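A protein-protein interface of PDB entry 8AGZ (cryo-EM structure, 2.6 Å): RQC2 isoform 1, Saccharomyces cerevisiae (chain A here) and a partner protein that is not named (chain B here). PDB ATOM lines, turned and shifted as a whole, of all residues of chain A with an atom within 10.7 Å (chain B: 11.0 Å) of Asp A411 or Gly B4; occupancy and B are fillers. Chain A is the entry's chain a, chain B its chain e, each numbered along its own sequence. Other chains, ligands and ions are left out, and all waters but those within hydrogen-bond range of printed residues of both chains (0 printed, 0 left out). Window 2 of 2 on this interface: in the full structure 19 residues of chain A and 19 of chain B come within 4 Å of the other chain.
NE2 of Gln A412 sits at hydrogen-bond distance from O of Ile B6 (3.0 Å).
The side-chain amide nitrogen (NE2) of Gln A412 lies within hydrogen-bond range of the side-chain amide oxygen (OD1) of Asn B7 (3.0 Å).
O of Asp A411 sits close to O of Gly B4 (3.2 Å).
ND2 of Asn B7 sits at hydrogen-bond distance from OD1 of Asp B35.
Ala A405 touches Thr B8 (CA to OG1, 3.3 Å).
Phe B9 touches Ala A405.
Gly B5 touches Gly A408 (CA to O, 3.9 Å).
O of Gly A408 touches O of Ile B6, 3.7 Å away.
CD2 of Leu A409 touches CD2 of Phe B9, at 3.6 Å.
CB of Asp A411 touches CA of Gly B5, at 3.97 Å.
Gly B4 touches Gln A412 (O to CA, 3.5 Å).
Gln A412 touches Gly B5 (CG to CA, 3.8 Å).
CG of Gln A412 touches CG of Pro B36, 3.9 Å away.
Met A414 touches Leu B33 (CE to CD1, 3.9 Å).
Of the printed residues of chain B, Ala A405 touches Thr B8 and Phe B9.
No residue of chain B comes within 4 Å of Gln A407.
Of chain B, only Gly B5 (3.9 Å) and Ile B6 (3.7 Å) come within 4 Å of Gly A408.
Of the printed residues of chain B, Leu A409 touches Phe B9.
Leu A443 touches none of the printed residues of chain B.
Gly B4 touches just these residues of chain A: Asp A411 and Gln A412.
Printed residues of chain A within 4 Å of Asn B7: Gln A412 (3.0 Å).
Printed residues of chain A within 4 Å of Phe B9: Ala A405 (3.6 Å) and Leu A409 (3.6 Å).
Of the printed residues of chain A, Leu B33 touches Met A414.
Lys B52 touches none of the printed residues of chain A.
The nearest residue of chain B that does not touch Asp A411 is Ile B6 (5.6 Å).
The nearest printed residue of chain A that does not touch Gly B4 is Gly A408 (5.5 Å).
The nearest printed residue of chain A that does not touch Phe B9 is Val A406 (4.6 Å).
Along chain A the printed residues that touch a printed residue of chain B span positions 405 to 414.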
ATOM      1  N   LYS A 403      -0.617  -8.776  32.476  1.00  0.00           N
ATOM      2  CA  LYS A 403       0.251  -8.427  31.354  1.00  0.00           C
ATOM      3  C   LYS A 403       0.302  -9.524  30.306  1.00  0.00           C
ATOM      4  O   LYS A 403       0.268  -9.235  29.105  1.00  0.00           O
ATOM      5  CB  LYS A 403       1.660  -8.156  31.850  1.00  0.00           C
ATOM      6  CG  LYS A 403       1.848  -6.911  32.656  1.00  0.00           C
ATOM      7  CD  LYS A 403       3.253  -6.958  33.146  1.00  0.00           C
ATOM      8  CE  LYS A 403       4.206  -6.751  32.005  1.00  0.00           C
ATOM      9  NZ  LYS A 403       5.557  -6.699  32.544  1.00  0.00           N
ATOM     10  N   LEU A 404       0.405 -10.783  30.741  1.00  0.00           N
ATOM     11  CA  LEU A 404       0.417 -11.895  29.799  1.00  0.00           C
ATOM     12  C   LEU A 404      -0.908 -11.998  29.060  1.00  0.00           C
ATOM     13  O   LEU A 404      -0.931 -12.302  27.864  1.00  0.00           O
ATOM     14  CB  LEU A 404       0.735 -13.198  30.526  1.00  0.00           C
ATOM     15  CG  LEU A 404       2.224 -13.518  30.659  1.00  0.00           C
ATOM     16  CD1 LEU A 404       2.422 -14.904  31.241  1.00  0.00           C
ATOM     17  CD2 LEU A 404       2.935 -13.392  29.319  1.00  0.00           C
ATOM     18  N   ALA A 405      -2.010 -11.682  29.743  1.00  0.00           N
ATOM     19  CA  ALA A 405      -3.314 -11.703  29.091  1.00  0.00           C
ATOM     20  C   ALA A 405      -3.442 -10.611  28.031  1.00  0.00           C
ATOM     21  O   ALA A 405      -3.847 -10.886  26.889  1.00  0.00           O
ATOM     22  CB  ALA A 405      -4.412 -11.571  30.142  1.00  0.00           C
ATOM     23  N   VAL A 406      -3.077  -9.374  28.381  1.00  0.00           N
ATOM     24  CA  VAL A 406      -3.193  -8.262  27.439  1.00  0.00           C
ATOM     25  C   VAL A 406      -2.222  -8.441  26.278  1.00  0.00           C
ATOM     26  O   VAL A 406      -2.563  -8.170  25.122  1.00  0.00           O
ATOM     27  CB  VAL A 406      -2.987  -6.917  28.167  1.00  0.00           C
ATOM     28  CG1 VAL A 406      -3.072  -5.745  27.199  1.00  0.00           C
ATOM     29  CG2 VAL A 406      -4.032  -6.742  29.245  1.00  0.00           C
ATOM     30  N   GLN A 407      -1.021  -8.956  26.553  1.00  0.00           N
ATOM     31  CA  GLN A 407      -0.060  -9.206  25.486  1.00  0.00           C
ATOM     32  C   GLN A 407      -0.498 -10.348  24.578  1.00  0.00           C
ATOM     33  O   GLN A 407      -0.230 -10.308  23.374  1.00  0.00           O
ATOM     34  CB  GLN A 407       1.315  -9.500  26.081  1.00  0.00           C
ATOM     35  CG  GLN A 407       2.446  -9.401  25.083  1.00  0.00           C
ATOM     36  CD  GLN A 407       2.873  -7.973  24.843  1.00  0.00           C
ATOM     37  OE1 GLN A 407       2.773  -7.462  23.727  1.00  0.00           O
ATOM     38  NE2 GLN A 407       3.346  -7.313  25.890  1.00  0.00           N
ATOM     39  N   GLY A 408      -1.181 -11.358  25.125  1.00  0.00           N
ATOM     40  CA  GLY A 408      -1.734 -12.401  24.279  1.00  0.00           C
ATOM     41  C   GLY A 408      -2.838 -11.890  23.372  1.00  0.00           C
ATOM     42  O   GLY A 408      -2.950 -12.317  22.221  1.00  0.00           O
ATOM     43  N   LEU A 409      -3.664 -10.970  23.874  1.00  0.00           N
ATOM     44  CA  LEU A 409      -4.648 -10.337  22.997  1.00  0.00           C
ATOM     45  C   LEU A 409      -3.993  -9.417  21.969  1.00  0.00           C
ATOM     46  O   LEU A 409      -4.501  -9.277  20.851  1.00  0.00           O
ATOM     47  CB  LEU A 409      -5.706  -9.580  23.801  1.00  0.00           C
ATOM     48  CG  LEU A 409      -6.917 -10.339  24.363  1.00  0.00           C
ATOM     49  CD1 LEU A 409      -7.702 -10.850  23.180  1.00  0.00           C
ATOM     50  CD2 LEU A 409      -6.616 -11.500  25.283  1.00  0.00           C
ATOM     51  N   ILE A 410      -2.883  -8.771  22.332  1.00  0.00           N
ATOM     52  CA  ILE A 410      -2.174  -7.901  21.393  1.00  0.00           C
ATOM     53  C   ILE A 410      -1.532  -8.716  20.275  1.00  0.00           C
ATOM     54  O   ILE A 410      -1.603  -8.345  19.096  1.00  0.00           O
ATOM     55  CB  ILE A 410      -1.149  -7.035  22.150  1.00  0.00           C
ATOM     56  CG1 ILE A 410      -1.863  -5.905  22.891  1.00  0.00           C
ATOM     57  CG2 ILE A 410      -0.066  -6.486  21.236  1.00  0.00           C
ATOM     58  CD1 ILE A 410      -0.940  -5.003  23.663  1.00  0.00           C
ATOM     59  N   ASP A 411      -0.961  -9.873  20.616  1.00  0.00           N
ATOM     60  CA  ASP A 411      -0.249 -10.697  19.644  1.00  0.00           C
ATOM     61  C   ASP A 411      -1.167 -11.379  18.639  1.00  0.00           C
ATOM     62  O   ASP A 411      -0.668 -11.967  17.676  1.00  0.00           O
ATOM     63  CB  ASP A 411       0.584 -11.750  20.369  1.00  0.00           C
ATOM     64  CG  ASP A 411       1.762 -11.150  21.100  1.00  0.00           C
ATOM     65  OD1 ASP A 411       2.068  -9.963  20.859  1.00  0.00           O
ATOM     66  OD2 ASP A 411       2.379 -11.859  21.919  1.00  0.00           O
ATOM     67  N   GLN A 412      -2.481 -11.313  18.827  1.00  0.00           N
ATOM     68  CA  GLN A 412      -3.438 -11.755  17.827  1.00  0.00           C
ATOM     69  C   GLN A 412      -3.724 -10.686  16.784  1.00  0.00           C
ATOM     70  O   GLN A 412      -4.578 -10.915  15.918  1.00  0.00           O
ATOM     71  CB  GLN A 412      -4.747 -12.174  18.499  1.00  0.00           C
ATOM     72  CG  GLN A 412      -4.582 -13.291  19.503  1.00  0.00           C
ATOM     73  CD  GLN A 412      -5.879 -13.650  20.190  1.00  0.00           C
ATOM     74  OE1 GLN A 412      -6.964 -13.400  19.663  1.00  0.00           O
ATOM     75  NE2 GLN A 412      -5.777 -14.236  21.377  1.00  0.00           N
ATOM     76  N   GLN A 413      -3.027  -9.542  16.862  1.00  0.00           N
ATOM     77  CA  GLN A 413      -3.217  -8.378  15.987  1.00  0.00           C
ATOM     78  C   GLN A 413      -4.659  -7.886  16.027  1.00  0.00           C
ATOM     79  O   GLN A 413      -5.253  -7.554  15.002  1.00  0.00           O
ATOM     80  CB  GLN A 413      -2.771  -8.669  14.553  1.00  0.00           C
ATOM     81  CG  GLN A 413      -1.283  -8.538  14.335  1.00  0.00           C
ATOM     82  CD  GLN A 413      -0.922  -8.571  12.871  1.00  0.00           C
ATOM     83  OE1 GLN A 413      -0.435  -9.580  12.366  1.00  0.00           O
ATOM     84  NE2 GLN A 413      -1.172  -7.470  12.176  1.00  0.00           N
ATOM     85  N   MET A 414      -5.229  -7.865  17.224  1.00  0.00           N
ATOM     86  CA  MET A 414      -6.623  -7.504  17.390  1.00  0.00           C
ATOM     87  C   MET A 414      -6.743  -5.993  17.547  1.00  0.00           C
ATOM     88  O   MET A 414      -5.834  -5.330  18.053  1.00  0.00           O
ATOM     89  CB  MET A 414      -7.202  -8.249  18.598  1.00  0.00           C
ATOM     90  CG  MET A 414      -8.691  -8.092  18.848  1.00  0.00           C
ATOM     91  SD  MET A 414      -9.230  -9.032  20.283  1.00  0.00           S
ATOM     92  CE  MET A 414      -9.113 -10.696  19.633  1.00  0.00           C
ATOM     93  N   ASP A 415      -7.867  -5.452  17.084  1.00  0.00           N
ATOM     94  CA  ASP A 415      -8.123  -4.023  17.149  1.00  0.00           C
ATOM     95  C   ASP A 415      -8.246  -3.566  18.598  1.00  0.00           C
ATOM     96  O   ASP A 415      -8.807  -4.265  19.444  1.00  0.00           O
ATOM     97  CB  ASP A 415      -9.397  -3.686  16.376  1.00  0.00           C
ATOM     98  CG  ASP A 415      -9.648  -2.199  16.277  1.00  0.00           C
ATOM     99  OD1 ASP A 415      -8.690  -1.412  16.426  1.00  0.00           O
ATOM    100  OD2 ASP A 415     -10.811  -1.811  16.053  1.00  0.00           O
ATOM    101  N   TRP A 416      -7.701  -2.374  18.874  1.00  0.00           N
ATOM    102  CA  TRP A 416      -7.588  -1.890  20.248  1.00  0.00           C
ATOM    103  C   TRP A 416      -8.946  -1.601  20.869  1.00  0.00           C
ATOM    104  O   TRP A 416      -9.164  -1.881  22.056  1.00  0.00           O
ATOM    105  CB  TRP A 416      -6.711  -0.636  20.289  1.00  0.00           C
ATOM    106  CG  TRP A 416      -5.265  -0.890  19.989  1.00  0.00           C
ATOM    107  CD1 TRP A 416      -4.666  -2.100  19.815  1.00  0.00           C
ATOM    108  CD2 TRP A 416      -4.228   0.091  19.860  1.00  0.00           C
ATOM    109  NE1 TRP A 416      -3.327  -1.937  19.571  1.00  0.00           N
ATOM    110  CE2 TRP A 416      -3.033  -0.601  19.594  1.00  0.00           C
ATOM    111  CE3 TRP A 416      -4.196   1.485  19.937  1.00  0.00           C
ATOM    112  CZ2 TRP A 416      -1.820   0.052  19.407  1.00  0.00           C
ATOM    113  CZ3 TRP A 416      -2.988   2.131  19.752  1.00  0.00           C
ATOM    114  CH2 TRP A 416      -1.819   1.414  19.488  1.00  0.00           C
ATOM    115  N   ILE A 419     -10.495  -4.805  21.752  1.00  0.00           N
ATOM    116  CA  ILE A 419      -9.888  -5.298  22.985  1.00  0.00           C
ATOM    117  C   ILE A 419     -10.502  -4.609  24.201  1.00  0.00           C
ATOM    118  O   ILE A 419     -10.815  -5.274  25.196  1.00  0.00           O
ATOM    119  CB  ILE A 419      -8.359  -5.121  22.935  1.00  0.00           C
ATOM    120  CG1 ILE A 419      -7.746  -6.097  21.930  1.00  0.00           C
ATOM    121  CG2 ILE A 419      -7.719  -5.332  24.298  1.00  0.00           C
ATOM    122  CD1 ILE A 419      -6.240  -5.984  21.801  1.00  0.00           C
ATOM    123  N   LEU A 443      -2.481   1.995  24.876  1.00  0.00           N
ATOM    124  CA  LEU A 443      -1.748   1.050  24.040  1.00  0.00           C
ATOM    125  C   LEU A 443      -0.869   1.743  23.010  1.00  0.00           C
ATOM    126  O   LEU A 443       0.019   1.102  22.442  1.00  0.00           O
ATOM    127  CB  LEU A 443      -2.721   0.104  23.340  1.00  0.00           C
ATOM    128  CG  LEU A 443      -3.639  -0.711  24.247  1.00  0.00           C
ATOM    129  CD1 LEU A 443      -4.368  -1.764  23.439  1.00  0.00           C
ATOM    130  CD2 LEU A 443      -2.841  -1.365  25.363  1.00  0.00           C
ATOM    131  N   ASN A 446       2.204   1.714  24.785  1.00  0.00           N
ATOM    132  CA  ASN A 446       2.409   0.360  25.321  1.00  0.00           C
ATOM    133  C   ASN A 446       2.272   0.318  26.841  1.00  0.00           C
ATOM    134  O   ASN A 446       3.058  -0.328  27.538  1.00  0.00           O
ATOM    135  CB  ASN A 446       3.761  -0.208  24.876  1.00  0.00           C
ATOM    136  CG  ASN A 446       3.749  -1.715  24.756  1.00  0.00           C
ATOM    137  OD1 ASN A 446       2.828  -2.294  24.186  1.00  0.00           O
ATOM    138  ND2 ASN A 446       4.786  -2.357  25.277  1.00  0.00           N
ATOM    139  N   LEU A 510       4.069  -2.462  29.253  1.00  0.00           N
ATOM    140  CA  LEU A 510       3.963  -3.846  28.814  1.00  0.00           C
ATOM    141  C   LEU A 510       5.297  -4.442  28.385  1.00  0.00           C
ATOM    142  O   LEU A 510       5.431  -5.670  28.386  1.00  0.00           O
ATOM    143  CB  LEU A 510       2.962  -3.953  27.665  1.00  0.00           C
ATOM    144  CG  LEU A 510       1.492  -3.982  28.070  1.00  0.00           C
ATOM    145  CD1 LEU A 510       0.618  -3.708  26.867  1.00  0.00           C
ATOM    146  CD2 LEU A 510       1.148  -5.317  28.691  1.00  0.00           C
ATOM    147  N   GLY A 511       6.280  -3.618  28.034  1.00  0.00           N
ATOM    148  CA  GLY A 511       7.567  -4.092  27.575  1.00  0.00           C
ATOM    149  C   GLY A 511       8.608  -4.295  28.653  1.00  0.00           C
ATOM    150  O   GLY A 511       9.744  -4.663  28.334  1.00  0.00           O
ATOM    151  N   SER B   2       2.244 -19.315  11.592  1.00  0.00           N
ATOM    152  CA  SER B   2       1.445 -18.422  10.768  1.00  0.00           C
ATOM    153  C   SER B   2       0.445 -17.659  11.621  1.00  0.00           C
ATOM    154  O   SER B   2       0.216 -16.474  11.397  1.00  0.00           O
ATOM    155  CB  SER B   2       0.721 -19.215   9.682  1.00  0.00           C
ATOM    156  OG  SER B   2      -0.120 -18.375   8.913  1.00  0.00           O
ATOM    157  N   PHE B   3      -0.143 -18.329  12.606  1.00  0.00           N
ATOM    158  CA  PHE B   3      -1.122 -17.690  13.474  1.00  0.00           C
ATOM    159  C   PHE B   3      -0.521 -17.518  14.849  1.00  0.00           C
ATOM    160  O   PHE B   3       0.065 -18.452  15.386  1.00  0.00           O
ATOM    161  CB  PHE B   3      -2.373 -18.544  13.584  1.00  0.00           C
ATOM    162  CG  PHE B   3      -3.210 -18.568  12.343  1.00  0.00           C
ATOM    163  CD1 PHE B   3      -4.088 -17.537  12.068  1.00  0.00           C
ATOM    164  CD2 PHE B   3      -3.135 -19.630  11.463  1.00  0.00           C
ATOM    165  CE1 PHE B   3      -4.870 -17.561  10.933  1.00  0.00           C
ATOM    166  CE2 PHE B   3      -3.913 -19.661  10.326  1.00  0.00           C
ATOM    167  CZ  PHE B   3      -4.785 -18.628  10.061  1.00  0.00           C
ATOM    168  N   GLY B   4      -0.658 -16.337  15.435  1.00  0.00           N
ATOM    169  CA  GLY B   4      -0.025 -16.082  16.715  1.00  0.00           C
ATOM    170  C   GLY B   4      -0.937 -15.518  17.776  1.00  0.00           C
ATOM    171  O   GLY B   4      -1.962 -14.922  17.461  1.00  0.00           O
ATOM    172  N   GLY B   5      -0.570 -15.700  19.038  1.00  0.00           N
ATOM    173  CA  GLY B   5      -1.375 -15.200  20.139  1.00  0.00           C
ATOM    174  C   GLY B   5      -2.223 -16.264  20.795  1.00  0.00           C
ATOM    175  O   GLY B   5      -2.502 -17.297  20.195  1.00  0.00           O
ATOM    176  N   ILE B   6      -2.622 -16.032  22.039  1.00  0.00           N
ATOM    177  CA  ILE B   6      -3.399 -17.022  22.774  1.00  0.00           C
ATOM    178  C   ILE B   6      -4.616 -16.358  23.408  1.00  0.00           C
ATOM    179  O   ILE B   6      -4.518 -15.240  23.907  1.00  0.00           O
ATOM    180  CB  ILE B   6      -2.524 -17.704  23.853  1.00  0.00           C
ATOM    181  CG1 ILE B   6      -1.512 -18.651  23.210  1.00  0.00           C
ATOM    182  CG2 ILE B   6      -3.364 -18.507  24.832  1.00  0.00           C
ATOM    183  CD1 ILE B   6      -2.150 -19.840  22.525  1.00  0.00           C
ATOM    184  N   ASN B   7      -5.763 -17.029  23.387  1.00  0.00           N
ATOM    185  CA  ASN B   7      -6.963 -16.474  24.002  1.00  0.00           C
ATOM    186  C   ASN B   7      -7.016 -16.756  25.494  1.00  0.00           C
ATOM    187  O   ASN B   7      -7.839 -17.544  25.943  1.00  0.00           O
ATOM    188  CB  ASN B   7      -8.202 -17.041  23.322  1.00  0.00           C
ATOM    189  CG  ASN B   7      -8.588 -16.264  22.081  1.00  0.00           C
ATOM    190  OD1 ASN B   7      -8.539 -15.036  22.065  1.00  0.00           O
ATOM    191  ND2 ASN B   7      -8.993 -16.977  21.038  1.00  0.00           N
ATOM    192  N   THR B   8      -6.152 -16.104  26.260  1.00  0.00           N
ATOM    193  CA  THR B   8      -6.110 -16.303  27.711  1.00  0.00           C
ATOM    194  C   THR B   8      -7.367 -15.869  28.451  1.00  0.00           C
ATOM    195  O   THR B   8      -7.795 -16.532  29.388  1.00  0.00           O
ATOM    196  CB  THR B   8      -4.899 -15.588  28.334  1.00  0.00           C
ATOM    197  OG1 THR B   8      -4.750 -14.302  27.725  1.00  0.00           O
ATOM    198  CG2 THR B   8      -3.634 -16.389  28.106  1.00  0.00           C
ATOM    199  N   PHE B   9      -7.951 -14.750  28.046  1.00  0.00           N
ATOM    200  CA  PHE B   9      -9.132 -14.254  28.732  1.00  0.00           C
ATOM    201  C   PHE B   9     -10.284 -15.231  28.636  1.00  0.00           C
ATOM    202  O   PHE B   9     -11.002 -15.442  29.609  1.00  0.00           O
ATOM    203  CB  PHE B   9      -9.548 -12.886  28.203  1.00  0.00           C
ATOM    204  CG  PHE B   9      -9.028 -11.748  29.022  1.00  0.00           C
ATOM    205  CD1 PHE B   9      -9.565 -11.480  30.264  1.00  0.00           C
ATOM    206  CD2 PHE B   9      -8.001 -10.951  28.556  1.00  0.00           C
ATOM    207  CE1 PHE B   9      -9.090 -10.437  31.027  1.00  0.00           C
ATOM    208  CE2 PHE B   9      -7.522  -9.903  29.312  1.00  0.00           C
ATOM    209  CZ  PHE B   9      -8.065  -9.646  30.552  1.00  0.00           C
ATOM    210  N   LEU B  33     -13.849 -15.547  18.707  1.00  0.00           N
ATOM    211  CA  LEU B  33     -13.028 -15.638  17.520  1.00  0.00           C
ATOM    212  C   LEU B  33     -12.162 -16.862  17.688  1.00  0.00           C
ATOM    213  O   LEU B  33     -11.722 -17.159  18.795  1.00  0.00           O
ATOM    214  CB  LEU B  33     -12.194 -14.377  17.393  1.00  0.00           C
ATOM    215  CG  LEU B  33     -13.031 -13.111  17.229  1.00  0.00           C
ATOM    216  CD1 LEU B  33     -12.252 -11.873  17.637  1.00  0.00           C
ATOM    217  CD2 LEU B  33     -13.530 -12.994  15.799  1.00  0.00           C
ATOM    218  N   PRO B  34     -11.896 -17.580  16.593  1.00  0.00           N
ATOM    219  CA  PRO B  34     -11.159 -18.837  16.740  1.00  0.00           C
ATOM    220  C   PRO B  34      -9.762 -18.656  17.297  1.00  0.00           C
ATOM    221  O   PRO B  34      -9.100 -17.670  16.991  1.00  0.00           O
ATOM    222  CB  PRO B  34     -11.092 -19.365  15.316  1.00  0.00           C
ATOM    223  CG  PRO B  34     -12.248 -18.737  14.616  1.00  0.00           C
ATOM    224  CD  PRO B  34     -12.370 -17.371  15.217  1.00  0.00           C
ATOM    225  N   ASP B  35      -9.324 -19.594  18.126  1.00  0.00           N
ATOM    226  CA  ASP B  35      -8.005 -19.510  18.727  1.00  0.00           C
ATOM    227  C   ASP B  35      -6.944 -19.631  17.660  1.00  0.00           C
ATOM    228  O   ASP B  35      -7.055 -20.452  16.759  1.00  0.00           O
ATOM    229  CB  ASP B  35      -7.838 -20.641  19.736  1.00  0.00           C
ATOM    230  CG  ASP B  35      -6.880 -20.297  20.860  1.00  0.00           C
ATOM    231  OD1 ASP B  35      -6.675 -19.100  21.139  1.00  0.00           O
ATOM    232  OD2 ASP B  35      -6.343 -21.233  21.488  1.00  0.00           O
ATOM    233  N   PRO B  36      -5.888 -18.831  17.779  1.00  0.00           N
ATOM    234  CA  PRO B  36      -4.819 -18.883  16.790  1.00  0.00           C
ATOM    235  C   PRO B  36      -4.159 -20.243  16.739  1.00  0.00           C
ATOM    236  O   PRO B  36      -3.818 -20.715  15.662  1.00  0.00           O
ATOM    237  CB  PRO B  36      -3.847 -17.842  17.306  1.00  0.00           C
ATOM    238  CG  PRO B  36      -4.742 -16.804  17.884  1.00  0.00           C
ATOM    239  CD  PRO B  36      -5.842 -17.578  18.552  1.00  0.00           C
ATOM    240  N   SER B  37      -3.981 -20.871  17.885  1.00  0.00           N
ATOM    241  CA  SER B  37      -3.398 -22.192  17.902  1.00  0.00           C
ATOM    242  C   SER B  37      -4.267 -23.167  17.138  1.00  0.00           C
ATOM    243  O   SER B  37      -3.768 -23.999  16.387  1.00  0.00           O
ATOM    244  CB  SER B  37      -3.267 -22.661  19.338  1.00  0.00           C
ATOM    245  OG  SER B  37      -4.527 -22.677  19.981  1.00  0.00           O
ATOM    246  N   LEU B  38      -5.573 -23.066  17.317  1.00  0.00           N
ATOM    247  CA  LEU B  38      -6.481 -23.939  16.599  1.00  0.00           C
ATOM    248  C   LEU B  38      -6.373 -23.675  15.115  1.00  0.00           C
ATOM    249  O   LEU B  38      -6.384 -24.598  14.301  1.00  0.00           O
ATOM    250  CB  LEU B  38      -7.908 -23.693  17.068  1.00  0.00           C
ATOM    251  CG  LEU B  38      -8.906 -24.826  16.845  1.00  0.00           C
ATOM    252  CD1 LEU B  38      -8.381 -26.115  17.454  1.00  0.00           C
ATOM    253  CD2 LEU B  38     -10.259 -24.460  17.436  1.00  0.00           C
ATOM    254  N   LEU B  39      -6.267 -22.408  14.752  1.00  0.00           N
ATOM    255  CA  LEU B  39      -6.197 -22.051  13.350  1.00  0.00           C
ATOM    256  C   LEU B  39      -4.960 -22.639  12.723  1.00  0.00           C
ATOM    257  O   LEU B  39      -5.002 -23.118  11.597  1.00  0.00           O
ATOM    258  CB  LEU B  39      -6.210 -20.539  13.208  1.00  0.00           C
ATOM    259  CG  LEU B  39      -7.559 -19.870  13.459  1.00  0.00           C
ATOM    260  CD1 LEU B  39      -7.403 -18.381  13.714  1.00  0.00           C
ATOM    261  CD2 LEU B  39      -8.504 -20.134  12.299  1.00  0.00           C
ATOM    262  N   ASN B  40      -3.860 -22.626  13.456  1.00  0.00           N
ATOM    263  CA  ASN B  40      -2.618 -23.183  12.953  1.00  0.00           C
ATOM    264  C   ASN B  40      -2.813 -24.649  12.684  1.00  0.00           C
ATOM    265  O   ASN B  40      -2.257 -25.190  11.739  1.00  0.00           O
ATOM    266  CB  ASN B  40      -1.504 -23.002  13.976  1.00  0.00           C
ATOM    267  CG  ASN B  40      -0.647 -21.793  13.693  1.00  0.00           C
ATOM    268  OD1 ASN B  40      -0.557 -21.335  12.556  1.00  0.00           O
ATOM    269  ND2 ASN B  40       0.005 -21.277  14.726  1.00  0.00           N
ATOM    270  N   SER B  41      -3.605 -25.305  13.511  1.00  0.00           N
ATOM    271  CA  SER B  41      -3.790 -26.741  13.383  1.00  0.00           C
ATOM    272  C   SER B  41      -4.522 -27.145  12.125  1.00  0.00           C
ATOM    273  O   SER B  41      -4.552 -28.323  11.792  1.00  0.00           O
ATOM    274  CB  SER B  41      -4.518 -27.286  14.606  1.00  0.00           C
ATOM    275  OG  SER B  41      -3.891 -26.854  15.800  1.00  0.00           O
ATOM    276  N   LYS B  48      -6.486 -22.206   5.650  1.00  0.00           N
ATOM    277  CA  LYS B  48      -6.091 -21.183   6.596  1.00  0.00           C
ATOM    278  C   LYS B  48      -6.376 -19.816   6.032  1.00  0.00           C
ATOM    279  O   LYS B  48      -6.870 -18.943   6.732  1.00  0.00           O
ATOM    280  CB  LYS B  48      -4.610 -21.296   6.924  1.00  0.00           C
ATOM    281  CG  LYS B  48      -4.214 -22.590   7.607  1.00  0.00           C
ATOM    282  CD  LYS B  48      -2.779 -22.511   8.095  1.00  0.00           C
ATOM    283  CE  LYS B  48      -2.329 -23.827   8.699  1.00  0.00           C
ATOM    284  NZ  LYS B  48      -0.953 -23.727   9.258  1.00  0.00           N
ATOM    285  N   LYS B  52      -8.685 -16.529   7.351  1.00  0.00           N
ATOM    286  CA  LYS B  52      -8.182 -15.199   7.637  1.00  0.00           C
ATOM    287  C   LYS B  52      -9.049 -14.190   6.935  1.00  0.00           C
ATOM    288  O   LYS B  52      -9.373 -13.144   7.485  1.00  0.00           O
ATOM    289  CB  LYS B  52      -6.755 -15.022   7.154  1.00  0.00           C
ATOM    290  CG  LYS B  52      -5.741 -16.011   7.686  1.00  0.00           C
ATOM    291  CD  LYS B  52      -4.379 -15.739   7.068  1.00  0.00           C
ATOM    292  CE  LYS B  52      -3.378 -16.840   7.377  1.00  0.00           C
ATOM    293  NZ  LYS B  52      -2.032 -16.558   6.807  1.00  0.00           N
ATOM    294  N   LEU B  55     -12.226 -13.466   8.723  1.00  0.00           N
ATOM    295  CA  LEU B  55     -12.048 -12.554   9.836  1.00  0.00           C
ATOM    296  C   LEU B  55     -12.058 -11.095   9.409  1.00  0.00           C
ATOM    297  O   LEU B  55     -12.544 -10.249  10.145  1.00  0.00           O
ATOM    298  CB  LEU B  55     -10.771 -12.879  10.586  1.00  0.00           C
ATOM    299  CG  LEU B  55     -10.738 -14.270  11.215  1.00  0.00           C
ATOM    300  CD1 LEU B  55      -9.368 -14.572  11.798  1.00  0.00           C
ATOM    301  CD2 LEU B  55     -11.821 -14.402  12.273  1.00  0.00           C
